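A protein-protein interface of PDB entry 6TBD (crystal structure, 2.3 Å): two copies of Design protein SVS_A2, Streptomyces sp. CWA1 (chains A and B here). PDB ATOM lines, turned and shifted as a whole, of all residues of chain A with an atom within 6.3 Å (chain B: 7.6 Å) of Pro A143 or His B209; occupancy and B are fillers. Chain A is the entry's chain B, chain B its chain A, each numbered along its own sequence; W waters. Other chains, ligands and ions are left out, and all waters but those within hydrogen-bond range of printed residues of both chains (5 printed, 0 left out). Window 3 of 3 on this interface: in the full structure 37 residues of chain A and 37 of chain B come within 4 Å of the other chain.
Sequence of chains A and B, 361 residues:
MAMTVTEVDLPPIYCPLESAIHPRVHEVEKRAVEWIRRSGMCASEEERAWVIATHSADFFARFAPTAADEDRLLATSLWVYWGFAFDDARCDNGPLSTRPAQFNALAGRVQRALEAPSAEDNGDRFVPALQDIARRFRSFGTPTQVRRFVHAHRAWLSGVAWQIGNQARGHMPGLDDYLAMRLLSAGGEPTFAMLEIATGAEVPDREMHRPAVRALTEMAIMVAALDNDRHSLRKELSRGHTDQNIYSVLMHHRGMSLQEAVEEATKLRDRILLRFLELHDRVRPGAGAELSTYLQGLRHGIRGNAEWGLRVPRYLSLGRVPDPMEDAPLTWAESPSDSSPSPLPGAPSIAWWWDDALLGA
Among the printed residues, pairs that only touch across the chains: Pro A143 with His B209 (3.4 Å), Thr A144 with Asp B205 (3.3 Å), Thr A144 with His B209 (3.4 Å), Arg A147 with His B209 (3.5 Å), Arg A147 with Arg B214 (3.5 Å) and His A151 with His B151 (3.4 Å).
Water W2 lies within hydrogen-bond range of the side-chain carboxylate of Asp B205 and the guanidinium group of Arg A148. Water W4 bridges the backbone carbonyl oxygen of His A151 (2.7 Å) and a ring nitrogen (ND1) of His B151 (3.2 Å). Water W1 bridges O of His B151 and ND1 of His A151. Water W5 bridges a ring nitrogen (NE2) of His B209 (3.1 Å) and the backbone carbonyl oxygen of Thr A144 (3.4 Å). Water W3 bridges NE of Arg B214 (3.2 Å) and NH1 of Arg A147 (3.2 Å).
OD2 of Asp B205 is in salt-bridge range of NH2 of Arg A148 (3.4 Å).
His A151 touches its own counterpart, His B151. Of the 7 pairs that touch across the chains among the printed residues, 1 has its exchanged pair printed and touching as well.
Of chain A, only Pro A143, Thr A144 and Arg A147 come within 4 Å of His B209. Printed residues of chain B within 4 Å of His A151: His B151 (3.4 Å). Of the printed residues of chain A, Arg B214 touches Arg A147 (3.5 Å). Printed residues of chain B within 4 Å of Arg A147: His B209 and Arg B214. Of the printed residues of chain A, Asp B205 touches Thr A144 (3.3 Å) and Arg A148 (3.4 Å). Of the printed residues of chain B, Arg A148 touches Asp B205 (3.4 Å). Met B208 touches none of the printed residues of chain A. The nearest residue of chain B that does not touch Pro A143 is Pro B211 (4.2 Å). The nearest residue of chain A that does not touch His B209 is His A151 (5.3 Å). The nearest printed residue of chain A that does not touch His B151 is Arg A148 (5.8 Å).
Of the 17 printed residues of chain B, 4 touch a printed residue of chain A. Hydrophobic or aromatic side chains of chain B within 4 Å of the printed part of chain A: His B151 and His B209. Printed residues of chain A that touch a printed residue of chain B: Pro A143, Thr A144, Arg A147, Arg A148 and His A151. Among the printed residues, 7 pairs touch across the chains. Among the printed residues, Asp or Glu carboxylates within 4 Å of a Lys or Arg side-chain nitrogen of the other chain: Arg A148 with Asp B205 (3.4 Å).
NH2 of Arg B148 lies within salt-bridge range of OD1 of Asp B205 (2.7 Å). A ring nitrogen (NE2) of His B209 is in hydrogen-bond range of the side-chain carboxylate (OD1) of Asp B205 (3.1 Å).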
ATOM      1  N   GLY A 141       4.927 -24.508   2.072  1.00  0.00           N
ATOM      2  CA  GLY A 141       5.565 -25.389   3.002  1.00  0.00           C
ATOM      3  C   GLY A 141       6.524 -24.611   3.855  1.00  0.00           C
ATOM      4  O   GLY A 141       6.876 -23.440   3.545  1.00  0.00           O
ATOM      5  N   THR A 142       6.958 -25.259   4.926  1.00  0.00           N
ATOM      6  CA  THR A 142       7.898 -24.665   5.857  1.00  0.00           C
ATOM      7  C   THR A 142       9.259 -24.932   5.256  1.00  0.00           C
ATOM      8  O   THR A 142       9.370 -25.851   4.410  1.00  0.00           O
ATOM      9  CB  THR A 142       7.798 -25.336   7.234  1.00  0.00           C
ATOM     10  OG1 THR A 142       8.182 -26.723   7.136  1.00  0.00           O
ATOM     11  CG2 THR A 142       6.337 -25.243   7.741  1.00  0.00           C
ATOM     12  N   PRO A 143      10.295 -24.165   5.677  1.00  0.00           N
ATOM     13  CA  PRO A 143      11.638 -24.444   5.143  1.00  0.00           C
ATOM     14  C   PRO A 143      12.112 -25.890   5.348  1.00  0.00           C
ATOM     15  O   PRO A 143      12.817 -26.463   4.518  1.00  0.00           O
ATOM     16  CB  PRO A 143      12.514 -23.421   5.851  1.00  0.00           C
ATOM     17  CG  PRO A 143      11.551 -22.280   6.199  1.00  0.00           C
ATOM     18  CD  PRO A 143      10.263 -22.935   6.500  1.00  0.00           C
ATOM     19  N   THR A 144      11.683 -26.476   6.428  1.00  0.00           N
ATOM     20  CA  THR A 144      11.929 -27.854   6.667  1.00  0.00           C
ATOM     21  C   THR A 144      11.321 -28.786   5.613  1.00  0.00           C
ATOM     22  O   THR A 144      12.009 -29.691   5.121  1.00  0.00           O
ATOM     23  CB  THR A 144      11.420 -28.239   8.067  1.00  0.00           C
ATOM     24  OG1 THR A 144      12.210 -27.535   9.016  1.00  0.00           O
ATOM     25  CG2 THR A 144      11.587 -29.788   8.321  1.00  0.00           C
ATOM     26  N   GLN A 145      10.042 -28.603   5.296  1.00  0.00           N
ATOM     27  CA  GLN A 145       9.353 -29.451   4.272  1.00  0.00           C
ATOM     28  C   GLN A 145      10.036 -29.268   2.935  1.00  0.00           C
ATOM     29  O   GLN A 145      10.224 -30.236   2.192  1.00  0.00           O
ATOM     30  CB  GLN A 145       7.857 -29.128   4.165  1.00  0.00           C
ATOM     31  CG  GLN A 145       7.086 -29.499   5.426  1.00  0.00           C
ATOM     32  CD  GLN A 145       5.642 -29.039   5.388  1.00  0.00           C
ATOM     33  OE1 GLN A 145       5.355 -27.898   5.038  1.00  0.00           O
ATOM     34  NE2 GLN A 145       4.721 -29.924   5.733  1.00  0.00           N
ATOM     35  N   VAL A 146      10.513 -28.047   2.667  1.00  0.00           N
ATOM     36  CA  VAL A 146      11.224 -27.809   1.426  1.00  0.00           C
ATOM     37  C   VAL A 146      12.523 -28.572   1.353  1.00  0.00           C
ATOM     38  O   VAL A 146      12.832 -29.222   0.322  1.00  0.00           O
ATOM     39  CB  VAL A 146      11.343 -26.314   1.128  1.00  0.00           C
ATOM     40  CG1 VAL A 146      12.168 -26.041  -0.139  1.00  0.00           C
ATOM     41  CG2 VAL A 146       9.922 -25.744   0.906  1.00  0.00           C
ATOM     42  N   ARG A 147      13.273 -28.564   2.450  1.00  0.00           N
ATOM     43  CA  ARG A 147      14.532 -29.312   2.477  1.00  0.00           C
ATOM     44  C   ARG A 147      14.375 -30.777   2.259  1.00  0.00           C
ATOM     45  O   ARG A 147      15.177 -31.403   1.569  1.00  0.00           O
ATOM     46  CB  ARG A 147      15.336 -29.098   3.756  1.00  0.00           C
ATOM     47  CG  ARG A 147      16.038 -27.790   3.873  1.00  0.00           C
ATOM     48  CD  ARG A 147      16.898 -27.512   2.683  1.00  0.00           C
ATOM     49  NE  ARG A 147      18.193 -28.157   2.707  1.00  0.00           N
ATOM     50  CZ  ARG A 147      19.069 -28.013   1.701  1.00  0.00           C
ATOM     51  NH1 ARG A 147      18.740 -27.286   0.611  1.00  0.00           N
ATOM     52  NH2 ARG A 147      20.254 -28.587   1.785  1.00  0.00           N
ATOM     53  N   ARG A 148      13.365 -31.341   2.879  1.00  0.00           N
ATOM     54  CA  ARG A 148      13.047 -32.759   2.683  1.00  0.00           C
ATOM     55  C   ARG A 148      12.839 -33.087   1.219  1.00  0.00           C
ATOM     56  O   ARG A 148      13.417 -34.059   0.709  1.00  0.00           O
ATOM     57  CB  ARG A 148      11.817 -33.152   3.505  1.00  0.00           C
ATOM     58  CG  ARG A 148      12.078 -33.134   5.007  1.00  0.00           C
ATOM     59  CD  ARG A 148      10.802 -33.375   5.804  1.00  0.00           C
ATOM     60  NE  ARG A 148      11.093 -33.357   7.219  1.00  0.00           N
ATOM     61  CZ  ARG A 148      10.190 -33.460   8.185  1.00  0.00           C
ATOM     62  NH1 ARG A 148       8.884 -33.629   7.893  1.00  0.00           N
ATOM     63  NH2 ARG A 148      10.591 -33.389   9.448  1.00  0.00           N
ATOM     64  N   HIS A 151      16.307 -32.816  -0.702  1.00  0.00           N
ATOM     65  CA  HIS A 151      17.171 -33.980  -0.538  1.00  0.00           C
ATOM     66  C   HIS A 151      16.620 -35.230  -1.253  1.00  0.00           C
ATOM     67  O   HIS A 151      17.374 -36.002  -1.809  1.00  0.00           O
ATOM     68  CB  HIS A 151      17.336 -34.283   0.945  1.00  0.00           C
ATOM     69  CG  HIS A 151      18.091 -33.248   1.707  1.00  0.00           C
ATOM     70  ND1 HIS A 151      19.225 -32.642   1.210  1.00  0.00           N
ATOM     71  CD2 HIS A 151      17.924 -32.758   2.961  1.00  0.00           C
ATOM     72  CE1 HIS A 151      19.688 -31.773   2.094  1.00  0.00           C
ATOM     73  NE2 HIS A 151      18.936 -31.844   3.168  1.00  0.00           N
ATOM     74  N   THR B 144      17.598 -37.957  12.971  1.00  0.00           N
ATOM     75  CA  THR B 144      17.534 -36.713  12.248  1.00  0.00           C
ATOM     76  C   THR B 144      18.946 -36.208  11.891  1.00  0.00           C
ATOM     77  O   THR B 144      19.230 -35.908  10.738  1.00  0.00           O
ATOM     78  CB  THR B 144      16.796 -35.647  13.099  1.00  0.00           C
ATOM     79  OG1 THR B 144      15.427 -36.045  13.300  1.00  0.00           O
ATOM     80  CG2 THR B 144      16.876 -34.248  12.418  1.00  0.00           C
ATOM     81  N   ARG B 148      20.711 -35.808   8.244  1.00  0.00           N
ATOM     82  CA  ARG B 148      21.436 -34.599   7.820  1.00  0.00           C
ATOM     83  C   ARG B 148      22.835 -34.964   7.289  1.00  0.00           C
ATOM     84  O   ARG B 148      23.283 -34.438   6.303  1.00  0.00           O
ATOM     85  CB  ARG B 148      21.488 -33.551   8.959  1.00  0.00           C
ATOM     86  CG  ARG B 148      20.102 -32.981   9.374  1.00  0.00           C
ATOM     87  CD  ARG B 148      20.190 -32.010  10.539  1.00  0.00           C
ATOM     88  NE  ARG B 148      18.858 -31.510  10.995  1.00  0.00           N
ATOM     89  CZ  ARG B 148      18.638 -30.758  12.085  1.00  0.00           C
ATOM     90  NH1 ARG B 148      19.644 -30.317  12.848  1.00  0.00           N
ATOM     91  NH2 ARG B 148      17.417 -30.389  12.399  1.00  0.00           N
ATOM     92  N   HIS B 151      22.394 -36.962   3.966  1.00  0.00           N
ATOM     93  CA  HIS B 151      22.002 -36.117   2.862  1.00  0.00           C
ATOM     94  C   HIS B 151      23.189 -35.237   2.426  1.00  0.00           C
ATOM     95  O   HIS B 151      23.401 -35.024   1.237  1.00  0.00           O
ATOM     96  CB  HIS B 151      20.804 -35.239   3.255  1.00  0.00           C
ATOM     97  CG  HIS B 151      19.509 -35.962   3.293  1.00  0.00           C
ATOM     98  ND1 HIS B 151      19.164 -36.935   2.380  1.00  0.00           N
ATOM     99  CD2 HIS B 151      18.470 -35.851   4.135  1.00  0.00           C
ATOM    100  CE1 HIS B 151      17.975 -37.401   2.676  1.00  0.00           C
ATOM    101  NE2 HIS B 151      17.524 -36.740   3.719  1.00  0.00           N
ATOM    102  N   VAL B 203      20.413 -29.071  16.610  1.00  0.00           N
ATOM    103  CA  VAL B 203      19.770 -27.872  16.175  1.00  0.00           C
ATOM    104  C   VAL B 203      18.372 -28.298  15.701  1.00  0.00           C
ATOM    105  O   VAL B 203      18.266 -29.134  14.847  1.00  0.00           O
ATOM    106  CB  VAL B 203      20.517 -27.240  15.031  1.00  0.00           C
ATOM    107  CG1 VAL B 203      19.874 -25.931  14.580  1.00  0.00           C
ATOM    108  CG2 VAL B 203      21.972 -27.023  15.417  1.00  0.00           C
ATOM    109  N   PRO B 204      17.309 -27.696  16.236  1.00  0.00           N
ATOM    110  CA  PRO B 204      15.950 -28.033  15.807  1.00  0.00           C
ATOM    111  C   PRO B 204      15.735 -27.704  14.327  1.00  0.00           C
ATOM    112  O   PRO B 204      16.371 -26.803  13.836  1.00  0.00           O
ATOM    113  CB  PRO B 204      15.068 -27.180  16.724  1.00  0.00           C
ATOM    114  CG  PRO B 204      15.941 -26.641  17.804  1.00  0.00           C
ATOM    115  CD  PRO B 204      17.345 -26.648  17.278  1.00  0.00           C
ATOM    116  N   ASP B 205      14.904 -28.471  13.635  1.00  0.00           N
ATOM    117  CA  ASP B 205      14.594 -28.269  12.204  1.00  0.00           C
ATOM    118  C   ASP B 205      14.269 -26.778  11.865  1.00  0.00           C
ATOM    119  O   ASP B 205      14.819 -26.203  10.939  1.00  0.00           O
ATOM    120  CB  ASP B 205      13.452 -29.224  11.728  1.00  0.00           C
ATOM    121  CG  ASP B 205      13.993 -30.595  11.032  1.00  0.00           C
ATOM    122  OD1 ASP B 205      15.209 -30.868  10.942  1.00  0.00           O
ATOM    123  OD2 ASP B 205      13.197 -31.483  10.586  1.00  0.00           O
ATOM    124  N   ARG B 206      13.417 -26.165  12.662  1.00  0.00           N
ATOM    125  CA  ARG B 206      12.963 -24.814  12.422  1.00  0.00           C
ATOM    126  C   ARG B 206      14.120 -23.826  12.422  1.00  0.00           C
ATOM    127  O   ARG B 206      14.065 -22.850  11.738  1.00  0.00           O
ATOM    128  CB  ARG B 206      11.933 -24.371  13.472  1.00  0.00           C
ATOM    129  CG  ARG B 206      11.068 -23.210  13.011  1.00  0.00           C
ATOM    130  CD  ARG B 206      10.476 -22.473  14.210  1.00  0.00           C
ATOM    131  NE  ARG B 206       9.421 -21.515  13.832  1.00  0.00           N
ATOM    132  CZ  ARG B 206       8.164 -21.484  14.303  1.00  0.00           C
ATOM    133  NH1 ARG B 206       7.718 -22.368  15.200  1.00  0.00           N
ATOM    134  NH2 ARG B 206       7.327 -20.537  13.866  1.00  0.00           N
ATOM    135  N   GLU B 207      15.164 -24.096  13.190  1.00  0.00           N
ATOM    136  CA  GLU B 207      16.338 -23.232  13.207  1.00  0.00           C
ATOM    137  C   GLU B 207      17.331 -23.684  12.156  1.00  0.00           C
ATOM    138  O   GLU B 207      17.796 -22.881  11.359  1.00  0.00           O
ATOM    139  CB  GLU B 207      16.970 -23.211  14.604  1.00  0.00           C
ATOM    140  CG  GLU B 207      16.192 -22.387  15.644  1.00  0.00           C
ATOM    141  CD  GLU B 207      17.045 -22.125  16.892  1.00  0.00           C
ATOM    142  OE1 GLU B 207      17.570 -20.961  17.109  1.00  0.00           O
ATOM    143  OE2 GLU B 207      17.226 -23.131  17.616  1.00  0.00           O
ATOM    144  N   MET B 208      17.648 -24.966  12.135  1.00  0.00           N
ATOM    145  CA  MET B 208      18.633 -25.466  11.189  1.00  0.00           C
ATOM    146  C   MET B 208      18.268 -25.140   9.754  1.00  0.00           C
ATOM    147  O   MET B 208      19.159 -24.806   9.002  1.00  0.00           O
ATOM    148  CB  MET B 208      18.840 -26.964  11.301  1.00  0.00           C
ATOM    149  CG  MET B 208      19.909 -27.509  10.348  1.00  0.00           C
ATOM    150  SD  MET B 208      21.543 -26.734  10.554  1.00  0.00           S
ATOM    151  CE  MET B 208      22.314 -27.772  11.744  1.00  0.00           C
ATOM    152  N   HIS B 209      16.985 -25.210   9.369  1.00  0.00           N
ATOM    153  CA  HIS B 209      16.644 -25.030   7.984  1.00  0.00           C
ATOM    154  C   HIS B 209      16.227 -23.617   7.637  1.00  0.00           C
ATOM    155  O   HIS B 209      15.805 -23.372   6.524  1.00  0.00           O
ATOM    156  CB  HIS B 209      15.569 -26.029   7.579  1.00  0.00           C
ATOM    157  CG  HIS B 209      15.974 -27.460   7.758  1.00  0.00           C
ATOM    158  ND1 HIS B 209      17.136 -27.965   7.228  1.00  0.00           N
ATOM    159  CD2 HIS B 209      15.378 -28.486   8.408  1.00  0.00           C
ATOM    160  CE1 HIS B 209      17.231 -29.255   7.520  1.00  0.00           C
ATOM    161  NE2 HIS B 209      16.172 -29.596   8.227  1.00  0.00           N
ATOM    162  N   ARG B 210      16.348 -22.685   8.576  1.00  0.00           N
ATOM    163  CA  ARG B 210      16.140 -21.264   8.265  1.00  0.00           C
ATOM    164  C   ARG B 210      17.045 -20.903   7.112  1.00  0.00           C
ATOM    165  O   ARG B 210      18.244 -21.259   7.145  1.00  0.00           O
ATOM    166  CB  ARG B 210      16.524 -20.344   9.425  1.00  0.00           C
ATOM    167  CG  ARG B 210      15.562 -20.360  10.584  1.00  0.00           C
ATOM    168  CD  ARG B 210      16.125 -19.516  11.749  1.00  0.00           C
ATOM    169  NE  ARG B 210      16.404 -18.146  11.326  1.00  0.00           N
ATOM    170  CZ  ARG B 210      17.023 -17.225  12.076  1.00  0.00           C
ATOM    171  NH1 ARG B 210      17.468 -17.521  13.295  1.00  0.00           N
ATOM    172  NH2 ARG B 210      17.209 -16.007  11.572  1.00  0.00           N
ATOM    173  N   PRO B 211      16.478 -20.229   6.093  1.00  0.00           N
ATOM    174  CA  PRO B 211      17.271 -19.810   4.974  1.00  0.00           C
ATOM    175  C   PRO B 211      18.594 -19.097   5.388  1.00  0.00           C
ATOM    176  O   PRO B 211      19.665 -19.442   4.879  1.00  0.00           O
ATOM    177  CB  PRO B 211      16.292 -18.933   4.175  1.00  0.00           C
ATOM    178  CG  PRO B 211      14.977 -19.610   4.399  1.00  0.00           C
ATOM    179  CD  PRO B 211      15.037 -20.059   5.824  1.00  0.00           C
ATOM    180  N   ALA B 212      18.523 -18.192   6.344  1.00  0.00           N
ATOM    181  CA  ALA B 212      19.704 -17.533   6.875  1.00  0.00           C
ATOM    182  C   ALA B 212      20.813 -18.470   7.330  1.00  0.00           C
ATOM    183  O   ALA B 212      21.973 -18.207   7.095  1.00  0.00           O
ATOM    184  CB  ALA B 212      19.325 -16.620   7.990  1.00  0.00           C
ATOM    185  N   VAL B 213      20.444 -19.550   7.989  1.00  0.00           N
ATOM    186  CA  VAL B 213      21.400 -20.517   8.519  1.00  0.00           C
ATOM    187  C   VAL B 213      21.921 -21.407   7.411  1.00  0.00           C
ATOM    188  O   VAL B 213      23.074 -21.822   7.438  1.00  0.00           O
ATOM    189  CB  VAL B 213      20.707 -21.390   9.558  1.00  0.00           C
ATOM    190  CG1 VAL B 213      21.600 -22.510  10.030  1.00  0.00           C
ATOM    191  CG2 VAL B 213      20.339 -20.522  10.715  1.00  0.00           C
ATOM    192  N   ARG B 214      21.054 -21.736   6.447  1.00  0.00           N
ATOM    193  CA  ARG B 214      21.465 -22.455   5.255  1.00  0.00           C
ATOM    194  C   ARG B 214      22.540 -21.679   4.537  1.00  0.00           C
ATOM    195  O   ARG B 214      23.590 -22.241   4.184  1.00  0.00           O
ATOM    196  CB  ARG B 214      20.279 -22.720   4.351  1.00  0.00           C
ATOM    197  CG  ARG B 214      20.558 -23.663   3.181  1.00  0.00           C
ATOM    198  CD  ARG B 214      20.810 -25.108   3.633  1.00  0.00           C
ATOM    199  NE  ARG B 214      21.845 -25.603   2.809  1.00  0.00           N
ATOM    200  CZ  ARG B 214      22.935 -26.225   3.165  1.00  0.00           C
ATOM    201  NH1 ARG B 214      23.184 -26.607   4.394  1.00  0.00           N
ATOM    202  NH2 ARG B 214      23.736 -26.561   2.179  1.00  0.00           N
ATOM    203  N   ALA B 215      22.318 -20.378   4.397  1.00  0.00           N
ATOM    204  CA  ALA B 215      23.293 -19.476   3.803  1.00  0.00           C
ATOM    205  C   ALA B 215      24.609 -19.317   4.564  1.00  0.00           C
ATOM    206  O   ALA B 215      25.671 -19.249   3.949  1.00  0.00           O
ATOM    207  CB  ALA B 215      22.694 -18.119   3.547  1.00  0.00           C
ATOM    208  N   LEU B 291      21.846 -23.606  18.063  1.00  0.00           N
ATOM    209  CA  LEU B 291      22.207 -22.922  16.828  1.00  0.00           C
ATOM    210  C   LEU B 291      23.451 -22.062  17.040  1.00  0.00           C
ATOM    211  O   LEU B 291      24.370 -22.065  16.195  1.00  0.00           O
ATOM    212  CB  LEU B 291      21.060 -22.116  16.244  1.00  0.00           C
ATOM    213  CG  LEU B 291      21.397 -21.254  15.028  1.00  0.00           C
ATOM    214  CD1 LEU B 291      21.687 -22.137  13.838  1.00  0.00           C
ATOM    215  CD2 LEU B 291      20.298 -20.271  14.750  1.00  0.00           C
HETATM  216  O   HOH W   1      21.278 -34.456  -0.438  1.00  0.00           O
HETATM  217  O   HOH W   2      13.865 -32.906   8.366  1.00  0.00           O
HETATM  218  O   HOH W   3      20.954 -25.156  -0.191  1.00  0.00           O
HETATM  219  O   HOH W   4      19.780 -36.820  -0.790  1.00  0.00           O
HETATM  220  O   HOH W   5      14.797 -31.336   6.095  1.00  0.00           O
